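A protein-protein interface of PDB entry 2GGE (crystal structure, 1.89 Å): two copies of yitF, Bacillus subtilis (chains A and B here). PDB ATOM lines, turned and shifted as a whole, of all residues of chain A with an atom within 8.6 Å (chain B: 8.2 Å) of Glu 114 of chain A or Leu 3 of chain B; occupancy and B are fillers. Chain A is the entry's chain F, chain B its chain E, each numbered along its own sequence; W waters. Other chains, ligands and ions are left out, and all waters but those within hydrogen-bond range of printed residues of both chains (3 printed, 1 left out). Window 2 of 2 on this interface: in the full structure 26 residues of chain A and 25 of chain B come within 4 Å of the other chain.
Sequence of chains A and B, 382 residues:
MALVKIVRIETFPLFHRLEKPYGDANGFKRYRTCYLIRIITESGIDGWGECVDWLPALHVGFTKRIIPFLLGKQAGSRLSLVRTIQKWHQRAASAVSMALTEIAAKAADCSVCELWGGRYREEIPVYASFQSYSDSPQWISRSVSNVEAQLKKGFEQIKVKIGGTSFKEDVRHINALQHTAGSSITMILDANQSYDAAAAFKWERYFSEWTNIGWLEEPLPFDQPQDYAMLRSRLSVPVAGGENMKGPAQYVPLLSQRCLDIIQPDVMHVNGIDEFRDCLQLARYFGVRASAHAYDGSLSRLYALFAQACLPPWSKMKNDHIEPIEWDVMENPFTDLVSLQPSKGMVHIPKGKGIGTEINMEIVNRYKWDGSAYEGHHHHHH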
ATOM      1  N   ALA A 105       6.424   7.348   3.012  1.00  0.00           N
ATOM      2  CA  ALA A 105       5.760   6.587   4.041  1.00  0.00           C
ATOM      3  C   ALA A 105       5.442   5.181   3.471  1.00  0.00           C
ATOM      4  O   ALA A 105       5.647   4.163   4.144  1.00  0.00           O
ATOM      5  CB  ALA A 105       4.514   7.324   4.541  1.00  0.00           C
ATOM      6  N   ALA A 108       8.446   3.011   3.325  1.00  0.00           N
ATOM      7  CA  ALA A 108       8.887   2.659   4.672  1.00  0.00           C
ATOM      8  C   ALA A 108       7.922   1.662   5.279  1.00  0.00           C
ATOM      9  O   ALA A 108       8.098   1.275   6.428  1.00  0.00           O
ATOM     10  CB  ALA A 108       8.915   3.907   5.562  1.00  0.00           C
ATOM     11  N   ASP A 109       6.892   1.303   4.511  1.00  0.00           N
ATOM     12  CA  ASP A 109       5.819   0.431   4.935  1.00  0.00           C
ATOM     13  C   ASP A 109       5.196   0.941   6.214  1.00  0.00           C
ATOM     14  O   ASP A 109       5.001   0.187   7.179  1.00  0.00           O
ATOM     15  CB  ASP A 109       6.317  -1.018   5.089  1.00  0.00           C
ATOM     16  CG  ASP A 109       5.172  -2.036   5.283  1.00  0.00           C
ATOM     17  OD1 ASP A 109       4.052  -1.795   4.771  1.00  0.00           O
ATOM     18  OD2 ASP A 109       5.405  -3.080   5.953  1.00  0.00           O
ATOM     19  N   CYS A 110       4.861   2.233   6.224  1.00  0.00           N
ATOM     20  CA  CYS A 110       4.228   2.808   7.410  1.00  0.00           C
ATOM     21  C   CYS A 110       3.305   3.969   7.068  1.00  0.00           C
ATOM     22  O   CYS A 110       3.259   4.436   5.904  1.00  0.00           O
ATOM     23  CB  CYS A 110       5.290   3.240   8.435  1.00  0.00           C
ATOM     24  SG  CYS A 110       6.197   4.766   8.019  1.00  0.00           S
ATOM     25  N   SER A 111       2.565   4.429   8.086  1.00  0.00           N
ATOM     26  CA  SER A 111       1.717   5.604   7.912  1.00  0.00           C
ATOM     27  C   SER A 111       2.518   6.895   7.973  1.00  0.00           C
ATOM     28  O   SER A 111       3.668   6.917   8.398  1.00  0.00           O
ATOM     29  CB  SER A 111       0.604   5.618   8.945  1.00  0.00           C
ATOM     30  OG  SER A 111       1.146   5.700  10.249  1.00  0.00           O
ATOM     31  N   VAL A 112       1.894   7.969   7.529  1.00  0.00           N
ATOM     32  CA  VAL A 112       2.502   9.303   7.612  1.00  0.00           C
ATOM     33  C   VAL A 112       2.806   9.665   9.083  1.00  0.00           C
ATOM     34  O   VAL A 112       3.908  10.001   9.389  1.00  0.00           O
ATOM     35  CB  VAL A 112       1.685  10.391   6.833  1.00  0.00           C
ATOM     36  CG1 VAL A 112       2.213  11.803   7.155  1.00  0.00           C
ATOM     37  CG2 VAL A 112       1.700  10.115   5.289  1.00  0.00           C
ATOM     38  N   CYS A 113       1.855   9.532   9.992  1.00  0.00           N
ATOM     39  CA  CYS A 113       2.111   9.808  11.395  1.00  0.00           C
ATOM     40  C   CYS A 113       3.287   9.014  11.975  1.00  0.00           C
ATOM     41  O   CYS A 113       4.085   9.558  12.730  1.00  0.00           O
ATOM     42  CB  CYS A 113       0.854   9.605  12.209  1.00  0.00           C
ATOM     43  SG  CYS A 113      -0.531  10.754  11.751  1.00  0.00           S
ATOM     44  N   GLU A 114       3.385   7.725  11.653  1.00  0.00           N
ATOM     45  CA  GLU A 114       4.538   6.906  12.022  1.00  0.00           C
ATOM     46  C   GLU A 114       5.875   7.401  11.457  1.00  0.00           C
ATOM     47  O   GLU A 114       6.923   7.383  12.148  1.00  0.00           O
ATOM     48  CB  GLU A 114       4.323   5.454  11.552  1.00  0.00           C
ATOM     49  CG  GLU A 114       3.304   4.717  12.402  1.00  0.00           C
ATOM     50  CD  GLU A 114       2.970   3.300  11.872  1.00  0.00           C
ATOM     51  OE1 GLU A 114       3.036   3.041  10.628  1.00  0.00           O
ATOM     52  OE2 GLU A 114       2.623   2.468  12.731  1.00  0.00           O
ATOM     53  N   LEU A 115       5.854   7.786  10.182  1.00  0.00           N
ATOM     54  CA  LEU A 115       7.015   8.400   9.570  1.00  0.00           C
ATOM     55  C   LEU A 115       7.547   9.550  10.447  1.00  0.00           C
ATOM     56  O   LEU A 115       8.762   9.716  10.630  1.00  0.00           O
ATOM     57  CB  LEU A 115       6.681   8.880   8.171  1.00  0.00           C
ATOM     58  CG  LEU A 115       7.860   9.327   7.343  1.00  0.00           C
ATOM     59  CD1 LEU A 115       8.862   8.187   7.088  1.00  0.00           C
ATOM     60  CD2 LEU A 115       7.380   9.922   6.020  1.00  0.00           C
ATOM     61  N   TRP A 116       6.605  10.327  10.996  1.00  0.00           N
ATOM     62  CA  TRP A 116       6.907  11.527  11.778  1.00  0.00           C
ATOM     63  C   TRP A 116       7.273  11.275  13.255  1.00  0.00           C
ATOM     64  O   TRP A 116       7.637  12.195  13.956  1.00  0.00           O
ATOM     65  CB  TRP A 116       5.716  12.451  11.701  1.00  0.00           C
ATOM     66  CG  TRP A 116       5.492  13.077  10.347  1.00  0.00           C
ATOM     67  CD1 TRP A 116       6.388  13.138   9.304  1.00  0.00           C
ATOM     68  CD2 TRP A 116       4.298  13.775   9.901  1.00  0.00           C
ATOM     69  NE1 TRP A 116       5.811  13.790   8.241  1.00  0.00           N
ATOM     70  CE2 TRP A 116       4.546  14.217   8.590  1.00  0.00           C
ATOM     71  CE3 TRP A 116       3.057  14.078  10.496  1.00  0.00           C
ATOM     72  CZ2 TRP A 116       3.580  14.946   7.829  1.00  0.00           C
ATOM     73  CZ3 TRP A 116       2.100  14.811   9.723  1.00  0.00           C
ATOM     74  CH2 TRP A 116       2.374  15.205   8.401  1.00  0.00           C
ATOM     75  N   GLY A 117       7.143  10.044  13.733  1.00  0.00           N
ATOM     76  CA  GLY A 117       7.459   9.695  15.093  1.00  0.00           C
ATOM     77  C   GLY A 117       6.273   9.123  15.856  1.00  0.00           C
ATOM     78  O   GLY A 117       6.383   8.798  17.063  1.00  0.00           O
ATOM     79  N   GLY A 118       5.140   9.010  15.170  1.00  0.00           N
ATOM     80  CA  GLY A 118       3.957   8.381  15.762  1.00  0.00           C
ATOM     81  C   GLY A 118       3.005   9.391  16.385  1.00  0.00           C
ATOM     82  O   GLY A 118       3.445  10.387  16.919  1.00  0.00           O
ATOM     83  N   ARG A 119       1.710   9.104  16.350  1.00  0.00           N
ATOM     84  CA  ARG A 119       0.698   9.995  16.850  1.00  0.00           C
ATOM     85  C   ARG A 119       0.659  10.103  18.410  1.00  0.00           C
ATOM     86  O   ARG A 119       1.212   9.262  19.111  1.00  0.00           O
ATOM     87  CB  ARG A 119      -0.663   9.579  16.271  1.00  0.00           C
ATOM     88  CG  ARG A 119      -1.065   8.132  16.621  1.00  0.00           C
ATOM     89  CD  ARG A 119      -2.264   7.631  15.786  1.00  0.00           C
ATOM     90  NE  ARG A 119      -2.878   6.429  16.354  1.00  0.00           N
ATOM     91  CZ  ARG A 119      -3.037   6.158  17.659  1.00  0.00           C
ATOM     92  NH1 ARG A 119      -2.632   7.006  18.620  1.00  0.00           N
ATOM     93  NH2 ARG A 119      -3.620   5.004  18.017  1.00  0.00           N
ATOM     94  N   PHE A 306      -3.146  14.821  10.312  1.00  0.00           N
ATOM     95  CA  PHE A 306      -2.049  13.998  10.784  1.00  0.00           C
ATOM     96  C   PHE A 306      -1.116  14.820  11.707  1.00  0.00           C
ATOM     97  O   PHE A 306      -0.747  14.380  12.814  1.00  0.00           O
ATOM     98  CB  PHE A 306      -1.236  13.408   9.613  1.00  0.00           C
ATOM     99  CG  PHE A 306      -1.992  12.397   8.781  1.00  0.00           C
ATOM    100  CD1 PHE A 306      -2.956  11.578   9.356  1.00  0.00           C
ATOM    101  CD2 PHE A 306      -1.715  12.273   7.425  1.00  0.00           C
ATOM    102  CE1 PHE A 306      -3.639  10.641   8.589  1.00  0.00           C
ATOM    103  CE2 PHE A 306      -2.377  11.355   6.642  1.00  0.00           C
ATOM    104  CZ  PHE A 306      -3.348  10.520   7.224  1.00  0.00           C
ATOM    105  N   CYS A 310       0.018  14.373  15.682  1.00  0.00           N
ATOM    106  CA  CYS A 310       1.406  14.277  16.173  1.00  0.00           C
ATOM    107  C   CYS A 310       1.877  15.523  16.917  1.00  0.00           C
ATOM    108  O   CYS A 310       3.082  15.685  17.131  1.00  0.00           O
ATOM    109  CB  CYS A 310       2.386  14.063  15.007  1.00  0.00           C
ATOM    110  SG  CYS A 310       2.211  12.497  14.132  1.00  0.00           S
ATOM    111  N   ILE A 349      -8.622   9.825  12.823  1.00  0.00           N
ATOM    112  CA  ILE A 349      -7.452   9.798  11.946  1.00  0.00           C
ATOM    113  C   ILE A 349      -7.284   8.380  11.324  1.00  0.00           C
ATOM    114  O   ILE A 349      -7.193   7.406  12.070  1.00  0.00           O
ATOM    115  CB  ILE A 349      -6.162  10.217  12.756  1.00  0.00           C
ATOM    116  CG1 ILE A 349      -6.273  11.664  13.270  1.00  0.00           C
ATOM    117  CG2 ILE A 349      -4.853  10.005  12.015  1.00  0.00           C
ATOM    118  CD1 ILE A 349      -6.779  12.722  12.267  1.00  0.00           C
ATOM    119  N   PRO A 350      -7.275   8.270   9.968  1.00  0.00           N
ATOM    120  CA  PRO A 350      -6.796   7.061   9.286  1.00  0.00           C
ATOM    121  C   PRO A 350      -5.471   6.565   9.883  1.00  0.00           C
ATOM    122  O   PRO A 350      -4.564   7.369  10.110  1.00  0.00           O
ATOM    123  CB  PRO A 350      -6.542   7.552   7.857  1.00  0.00           C
ATOM    124  CG  PRO A 350      -7.557   8.582   7.659  1.00  0.00           C
ATOM    125  CD  PRO A 350      -7.754   9.266   8.996  1.00  0.00           C
ATOM    126  N   LYS A 351      -5.380   5.254  10.127  1.00  0.00           N
ATOM    127  CA  LYS A 351      -4.175   4.631  10.660  1.00  0.00           C
ATOM    128  C   LYS A 351      -3.362   3.909   9.596  1.00  0.00           C
ATOM    129  O   LYS A 351      -2.224   3.546   9.854  1.00  0.00           O
ATOM    130  CB  LYS A 351      -4.515   3.653  11.775  1.00  0.00           C
ATOM    131  CG  LYS A 351      -4.928   4.348  13.064  1.00  0.00           C
ATOM    132  CD  LYS A 351      -4.586   3.499  14.295  1.00  0.00           C
ATOM    133  CE  LYS A 351      -5.826   2.883  14.919  1.00  0.00           C
ATOM    134  NZ  LYS A 351      -6.768   3.926  15.378  1.00  0.00           N
ATOM    135  N   GLY A 352      -3.921   3.731   8.397  1.00  0.00           N
ATOM    136  CA  GLY A 352      -3.278   2.897   7.378  1.00  0.00           C
ATOM    137  C   GLY A 352      -1.950   3.433   6.865  1.00  0.00           C
ATOM    138  O   GLY A 352      -1.621   4.601   7.064  1.00  0.00           O
ATOM    139  N   LYS A 353      -1.189   2.574   6.191  1.00  0.00           N
ATOM    140  CA  LYS A 353       0.048   2.994   5.526  1.00  0.00           C
ATOM    141  C   LYS A 353      -0.217   4.058   4.488  1.00  0.00           C
ATOM    142  O   LYS A 353      -1.357   4.209   4.041  1.00  0.00           O
ATOM    143  CB  LYS A 353       0.771   1.786   4.943  1.00  0.00           C
ATOM    144  CG  LYS A 353       1.164   0.832   6.110  1.00  0.00           C
ATOM    145  CD  LYS A 353       1.188  -0.632   5.736  1.00  0.00           C
ATOM    146  CE  LYS A 353       1.508  -1.459   6.979  1.00  0.00           C
ATOM    147  NZ  LYS A 353       2.325  -2.710   6.646  1.00  0.00           N
ATOM    148  N   GLY A 354       0.832   4.806   4.131  1.00  0.00           N
ATOM    149  CA  GLY A 354       0.693   6.054   3.382  1.00  0.00           C
ATOM    150  C   GLY A 354      -0.257   6.980   4.117  1.00  0.00           C
ATOM    151  O   GLY A 354      -0.137   7.164   5.322  1.00  0.00           O
ATOM    152  N   LEU B   3       1.548  -2.194  16.246  1.00  0.00           N
ATOM    153  CA  LEU B   3       2.927  -2.353  15.633  1.00  0.00           C
ATOM    154  C   LEU B   3       3.919  -2.863  16.714  1.00  0.00           C
ATOM    155  O   LEU B   3       3.501  -3.196  17.828  1.00  0.00           O
ATOM    156  CB  LEU B   3       3.352  -1.048  14.897  1.00  0.00           C
ATOM    157  CG  LEU B   3       4.378  -0.821  13.760  1.00  0.00           C
ATOM    158  CD1 LEU B   3       5.188  -2.040  13.261  1.00  0.00           C
ATOM    159  CD2 LEU B   3       3.708  -0.166  12.561  1.00  0.00           C
ATOM    160  N   VAL B   4       5.209  -2.969  16.395  1.00  0.00           N
ATOM    161  CA  VAL B   4       6.123  -3.787  17.228  1.00  0.00           C
ATOM    162  C   VAL B   4       6.430  -3.203  18.625  1.00  0.00           C
ATOM    163  O   VAL B   4       6.502  -1.976  18.815  1.00  0.00           O
ATOM    164  CB  VAL B   4       7.409  -4.276  16.461  1.00  0.00           C
ATOM    165  CG1 VAL B   4       8.452  -4.808  17.432  1.00  0.00           C
ATOM    166  CG2 VAL B   4       7.054  -5.386  15.461  1.00  0.00           C
ATOM    167  N   LYS B   5       6.552  -4.106  19.592  1.00  0.00           N
ATOM    168  CA  LYS B   5       6.834  -3.762  20.944  1.00  0.00           C
ATOM    169  C   LYS B   5       8.316  -3.947  21.302  1.00  0.00           C
ATOM    170  O   LYS B   5       9.040  -4.793  20.732  1.00  0.00           O
ATOM    171  CB  LYS B   5       6.001  -4.623  21.898  1.00  0.00           C
ATOM    172  CG  LYS B   5       4.466  -4.451  21.899  1.00  0.00           C
ATOM    173  CD  LYS B   5       3.928  -5.479  22.914  1.00  0.00           C
ATOM    174  CE  LYS B   5       2.473  -5.877  22.660  1.00  0.00           C
ATOM    175  NZ  LYS B   5       2.253  -6.641  21.372  1.00  0.00           N
ATOM    176  N   ILE B   6       8.737  -3.155  22.285  1.00  0.00           N
ATOM    177  CA  ILE B   6      10.059  -3.244  22.901  1.00  0.00           C
ATOM    178  C   ILE B   6      10.066  -4.433  23.857  1.00  0.00           C
ATOM    179  O   ILE B   6       9.292  -4.468  24.823  1.00  0.00           O
ATOM    180  CB  ILE B   6      10.408  -1.935  23.696  1.00  0.00           C
ATOM    181  CG1 ILE B   6      10.664  -0.778  22.727  1.00  0.00           C
ATOM    182  CG2 ILE B   6      11.619  -2.126  24.664  1.00  0.00           C
ATOM    183  CD1 ILE B   6      10.610   0.584  23.408  1.00  0.00           C
ATOM    184  N   THR B  41      13.623  -4.877  19.759  1.00  0.00           N
ATOM    185  CA  THR B  41      12.172  -5.057  19.567  1.00  0.00           C
ATOM    186  C   THR B  41      11.799  -6.542  19.333  1.00  0.00           C
ATOM    187  O   THR B  41      12.684  -7.417  19.310  1.00  0.00           O
ATOM    188  CB  THR B  41      11.617  -4.186  18.409  1.00  0.00           C
ATOM    189  OG1 THR B  41      12.010  -4.742  17.158  1.00  0.00           O
ATOM    190  CG2 THR B  41      12.144  -2.739  18.496  1.00  0.00           C
ATOM    191  N   GLU B  42      10.495  -6.796  19.152  1.00  0.00           N
ATOM    192  CA  GLU B  42       9.956  -8.151  18.908  1.00  0.00           C
ATOM    193  C   GLU B  42      10.513  -8.769  17.656  1.00  0.00           C
ATOM    194  O   GLU B  42      10.999  -9.887  17.684  1.00  0.00           O
ATOM    195  CB  GLU B  42       8.439  -8.148  18.804  1.00  0.00           C
ATOM    196  CG  GLU B  42       7.752  -7.851  20.109  1.00  0.00           C
ATOM    197  CD  GLU B  42       6.266  -8.072  20.026  1.00  0.00           C
ATOM    198  OE1 GLU B  42       5.610  -7.433  19.126  1.00  0.00           O
ATOM    199  OE2 GLU B  42       5.771  -8.885  20.867  1.00  0.00           O
ATOM    200  N   SER B  43      10.443  -8.037  16.555  1.00  0.00           N
ATOM    201  CA  SER B  43      10.981  -8.504  15.292  1.00  0.00           C
ATOM    202  C   SER B  43      12.510  -8.712  15.280  1.00  0.00           C
ATOM    203  O   SER B  43      13.050  -9.165  14.256  1.00  0.00           O
ATOM    204  CB  SER B  43      10.593  -7.526  14.175  1.00  0.00           C
ATOM    205  OG  SER B  43      11.291  -6.307  14.341  1.00  0.00           O
ATOM    206  N   ILE B  45      14.598  -6.204  15.421  1.00  0.00           N
ATOM    207  CA  ILE B  45      15.180  -4.871  15.143  1.00  0.00           C
ATOM    208  C   ILE B  45      15.618  -4.181  16.460  1.00  0.00           C
ATOM    209  O   ILE B  45      14.848  -4.081  17.431  1.00  0.00           O
ATOM    210  CB  ILE B  45      14.248  -3.964  14.276  1.00  0.00           C
ATOM    211  CG1 ILE B  45      13.895  -4.676  12.960  1.00  0.00           C
ATOM    212  CG2 ILE B  45      14.966  -2.632  13.932  1.00  0.00           C
ATOM    213  CD1 ILE B  45      12.672  -4.132  12.236  1.00  0.00           C
ATOM    214  N   GLY B  72       7.430  -3.496  26.623  1.00  0.00           N
ATOM    215  CA  GLY B  72       6.065  -3.754  26.205  1.00  0.00           C
ATOM    216  C   GLY B  72       5.465  -2.554  25.510  1.00  0.00           C
ATOM    217  O   GLY B  72       4.260  -2.551  25.190  1.00  0.00           O
ATOM    218  N   LYS B  73       6.296  -1.531  25.258  1.00  0.00           N
ATOM    219  CA  LYS B  73       5.755  -0.336  24.658  1.00  0.00           C
ATOM    220  C   LYS B  73       5.942  -0.312  23.171  1.00  0.00           C
ATOM    221  O   LYS B  73       6.918  -0.841  22.624  1.00  0.00           O
ATOM    222  CB  LYS B  73       6.312   0.951  25.299  1.00  0.00           C
ATOM    223  CG  LYS B  73       5.939   1.232  26.759  1.00  0.00           C
ATOM    224  CD  LYS B  73       4.491   1.633  26.922  1.00  0.00           C
ATOM    225  CE  LYS B  73       4.175   2.052  28.349  1.00  0.00           C
ATOM    226  NZ  LYS B  73       4.581   0.994  29.303  1.00  0.00           N
ATOM    227  N   GLN B  74       4.966   0.315  22.531  1.00  0.00           N
ATOM    228  CA  GLN B  74       5.000   0.677  21.128  1.00  0.00           C
ATOM    229  C   GLN B  74       6.316   1.353  20.675  1.00  0.00           C
ATOM    230  O   GLN B  74       6.450   2.580  20.808  1.00  0.00           O
ATOM    231  CB  GLN B  74       3.875   1.690  20.865  1.00  0.00           C
ATOM    232  CG  GLN B  74       2.680   1.224  20.046  1.00  0.00           C
ATOM    233  CD  GLN B  74       3.053   0.040  19.256  1.00  0.00           C
ATOM    234  OE1 GLN B  74       2.834  -1.070  19.718  1.00  0.00           O
ATOM    235  NE2 GLN B  74       3.729   0.247  18.104  1.00  0.00           N
ATOM    236  N   ALA B  75       7.240   0.595  20.082  1.00  0.00           N
ATOM    237  CA  ALA B  75       8.489   1.198  19.582  1.00  0.00           C
ATOM    238  C   ALA B  75       8.305   2.329  18.570  1.00  0.00           C
ATOM    239  O   ALA B  75       9.203   3.149  18.403  1.00  0.00           O
ATOM    240  CB  ALA B  75       9.454   0.134  19.026  1.00  0.00           C
ATOM    241  N   GLY B  76       7.162   2.394  17.899  1.00  0.00           N
ATOM    242  CA  GLY B  76       6.942   3.408  16.873  1.00  0.00           C
ATOM    243  C   GLY B  76       6.397   4.722  17.440  1.00  0.00           C
ATOM    244  O   GLY B  76       6.212   5.702  16.687  1.00  0.00           O
ATOM    245  N   SER B  77       6.125   4.744  18.750  1.00  0.00           N
ATOM    246  CA  SER B  77       5.548   5.927  19.383  1.00  0.00           C
ATOM    247  C   SER B  77       6.673   6.797  19.961  1.00  0.00           C
ATOM    248  O   SER B  77       6.726   7.025  21.173  1.00  0.00           O
ATOM    249  CB  SER B  77       4.621   5.500  20.530  1.00  0.00           C
ATOM    250  OG  SER B  77       3.510   4.821  19.999  1.00  0.00           O
ATOM    251  N   ARG B  78       7.570   7.241  19.090  1.00  0.00           N
ATOM    252  CA  ARG B  78       8.806   7.840  19.541  1.00  0.00           C
ATOM    253  C   ARG B  78       8.488   9.153  20.250  1.00  0.00           C
ATOM    254  O   ARG B  78       8.860   9.364  21.425  1.00  0.00           O
ATOM    255  CB  ARG B  78       9.759   8.087  18.363  1.00  0.00           C
ATOM    256  CG  ARG B  78      11.155   8.462  18.839  1.00  0.00           C
ATOM    257  CD  ARG B  78      12.122   8.648  17.689  1.00  0.00           C
ATOM    258  NE  ARG B  78      11.764   9.777  16.817  1.00  0.00           N
ATOM    259  CZ  ARG B  78      11.247   9.657  15.594  1.00  0.00           C
ATOM    260  NH1 ARG B  78      11.035   8.447  15.076  1.00  0.00           N
ATOM    261  NH2 ARG B  78      10.956  10.761  14.873  1.00  0.00           N
ATOM    262  N   LEU B  79       7.721   9.990  19.567  1.00  0.00           N
ATOM    263  CA  LEU B  79       7.403  11.340  20.096  1.00  0.00           C
ATOM    264  C   LEU B  79       6.850  11.201  21.497  1.00  0.00           C
ATOM    265  O   LEU B  79       7.404  11.728  22.476  1.00  0.00           O
ATOM    266  CB  LEU B  79       6.420  12.050  19.174  1.00  0.00           C
ATOM    267  CG  LEU B  79       6.854  12.373  17.731  1.00  0.00           C
ATOM    268  CD1 LEU B  79       5.826  13.260  17.055  1.00  0.00           C
ATOM    269  CD2 LEU B  79       8.192  13.070  17.644  1.00  0.00           C
ATOM    270  N   ALA B 104      13.374   2.965  13.827  1.00  0.00           N
ATOM    271  CA  ALA B 104      12.539   3.549  12.796  1.00  0.00           C
ATOM    272  C   ALA B 104      13.190   3.470  11.438  1.00  0.00           C
ATOM    273  O   ALA B 104      12.540   3.033  10.465  1.00  0.00           O
ATOM    274  CB  ALA B 104      12.131   5.015  13.131  1.00  0.00           C
ATOM    275  N   ALA B 107      13.665  -0.405  10.199  1.00  0.00           N
ATOM    276  CA  ALA B 107      12.355  -0.886   9.844  1.00  0.00           C
ATOM    277  C   ALA B 107      11.888  -0.227   8.560  1.00  0.00           C
ATOM    278  O   ALA B 107      11.179  -0.856   7.787  1.00  0.00           O
ATOM    279  CB  ALA B 107      11.371  -0.660  10.999  1.00  0.00           C
ATOM    280  N   ALA B 108      12.316   1.013   8.293  1.00  0.00           N
ATOM    281  CA  ALA B 108      11.906   1.707   7.065  1.00  0.00           C
ATOM    282  C   ALA B 108      12.793   1.364   5.904  1.00  0.00           C
ATOM    283  O   ALA B 108      12.574   1.807   4.795  1.00  0.00           O
ATOM    284  CB  ALA B 108      11.903   3.214   7.271  1.00  0.00           C
ATOM    285  N   LEU B 115      15.040   9.070   6.506  1.00  0.00           N
ATOM    286  CA  LEU B 115      13.903   9.123   7.406  1.00  0.00           C
ATOM    287  C   LEU B 115      13.447  10.594   7.654  1.00  0.00           C
ATOM    288  O   LEU B 115      12.231  10.897   7.673  1.00  0.00           O
ATOM    289  CB  LEU B 115      14.254   8.457   8.737  1.00  0.00           C
ATOM    290  CG  LEU B 115      13.065   8.272   9.670  1.00  0.00           C
ATOM    291  CD1 LEU B 115      12.274   7.027   9.192  1.00  0.00           C
ATOM    292  CD2 LEU B 115      13.549   8.137  11.126  1.00  0.00           C
HETATM  293  O   HOH W   1       2.111   6.473  18.553  1.00  0.00           O
HETATM  294  O   HOH W   2      10.056   7.803  12.635  1.00  0.00           O
HETATM  295  O   HOH W   3      10.816  10.931  11.672  1.00  0.00           O
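Ala 108 of chain A touches its own counterpart, Ala 108 of chain B.
Of the 12 pairs that touch across the chains among the printed residues, 1 has its exchanged pair printed and touching as well.
Glu 114 of chain A touches just one residue of chain B: Leu 3 (2.9 Å).
Leu 3 of chain B touches one residue of chain A.
Printed residues of chain B within 4 Å of Ala 108 of chain A: Ala 107 and Ala 108.
Printed residues of chain A within 4 Å of Ser 77 of chain B: Gly 117 (3.5 Å).
Of the printed residues of chain A, Leu 79 of chain B touches Trp 116 (3.7 Å), Gly 117 (3.1 Å), Gly 118 (3.7 Å) and Cys 310 (3.7 Å).
Printed residues of chain A within 4 Å of Ala 107 of chain B: Ala 108.
Lys 73 of chain B touches none of the printed residues of chain A.
The nearest printed residue of chain A that does not touch Arg 78 of chain B is Leu 115 of chain A (4.9 Å).
Among the printed residues, pairs that only touch across the chains: Ala 108 of chain A with Ala 107 of chain B, Ala 108 of chain A with Ala 108 of chain B, Glu 114 of chain A with Leu 3 of chain B, Trp 116 of chain A with Arg 78 of chain B, Trp 116 of chain A with Leu 79 of chain B, Gly 117 of chain A with Ser 77 of chain B, Gly 118 of chain A with Gly 76 of chain B, Gly 118 of chain A with Leu 79 of chain B and Cys 310 of chain A with Leu 79 of chain B.
O of Leu 3 of chain B lies close to OE1 of Gln 74 of chain B, 2.9 Å away.
The side-chain carboxylate (OE1) of Glu 114 of chain A lies within hydrogen-bond range of the backbone NH (N) of Ser 111 of chain A, 2.9 Å away.
O of Cys 113 of chain A sits close to SG of Cys 310 of chain A (3.8 Å).
The backbone carbonyl oxygen of Gly 118 of chain A lies within hydrogen-bond range of the side-chain sulfur of Cys 310 of chain A (3.7 Å).
The backbone carbonyl oxygen (O) of Phe 306 of chain A is in hydrogen-bond range of the side-chain sulfur (SG) of Cys 310 of chain A (3.7 Å).
The backbone NH of Arg 78 of chain B sits at hydrogen-bond distance from the backbone carbonyl oxygen of Gly 117 of chain A (2.8 Å).
The backbone carbonyl oxygen (O) of Gly 117 of chain A lies within hydrogen-bond range of the backbone NH (N) of Leu 79 of chain B.
The backbone carbonyl oxygen of Gly 117 of chain A lies close to the backbone carbonyl oxygen of Gly 76 of chain B, 3.1 Å away.
Of the 21 printed residues of chain A, 6 touch a printed residue of chain B.
Hydrophobic or aromatic side chains of chain A within 4 Å of the printed part of chain B: Ala 108.
Of the 20 printed residues of chain B, 7 touch a printed residue of chain A.
Hydrophobic or aromatic side chains of chain B within 4 Å of the printed part of chain A: Leu 3, Leu 79 and Ala 108.
Among the printed residues, no Asp or Glu carboxylate lies within 4 Å of a Lys or Arg side-chain nitrogen of the other chain.
Water W1 lies within hydrogen-bond range of OG of Ser 77 of chain B and O of Arg 119 of chain A.
Water W3 bridges the backbone carbonyl oxygen (O) of Leu 115 of chain A (2.6 Å) and the guanidinium group (NH2) of Arg 78 of chain B (3.2 Å).
Water W2 lies within hydrogen-bond range of the guanidinium group (NH1) of Arg 78 of chain B, the backbone carbonyl oxygen (O) of Leu 115 of chain A and the backbone carbonyl oxygen (O) of Glu 114 of chain A.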
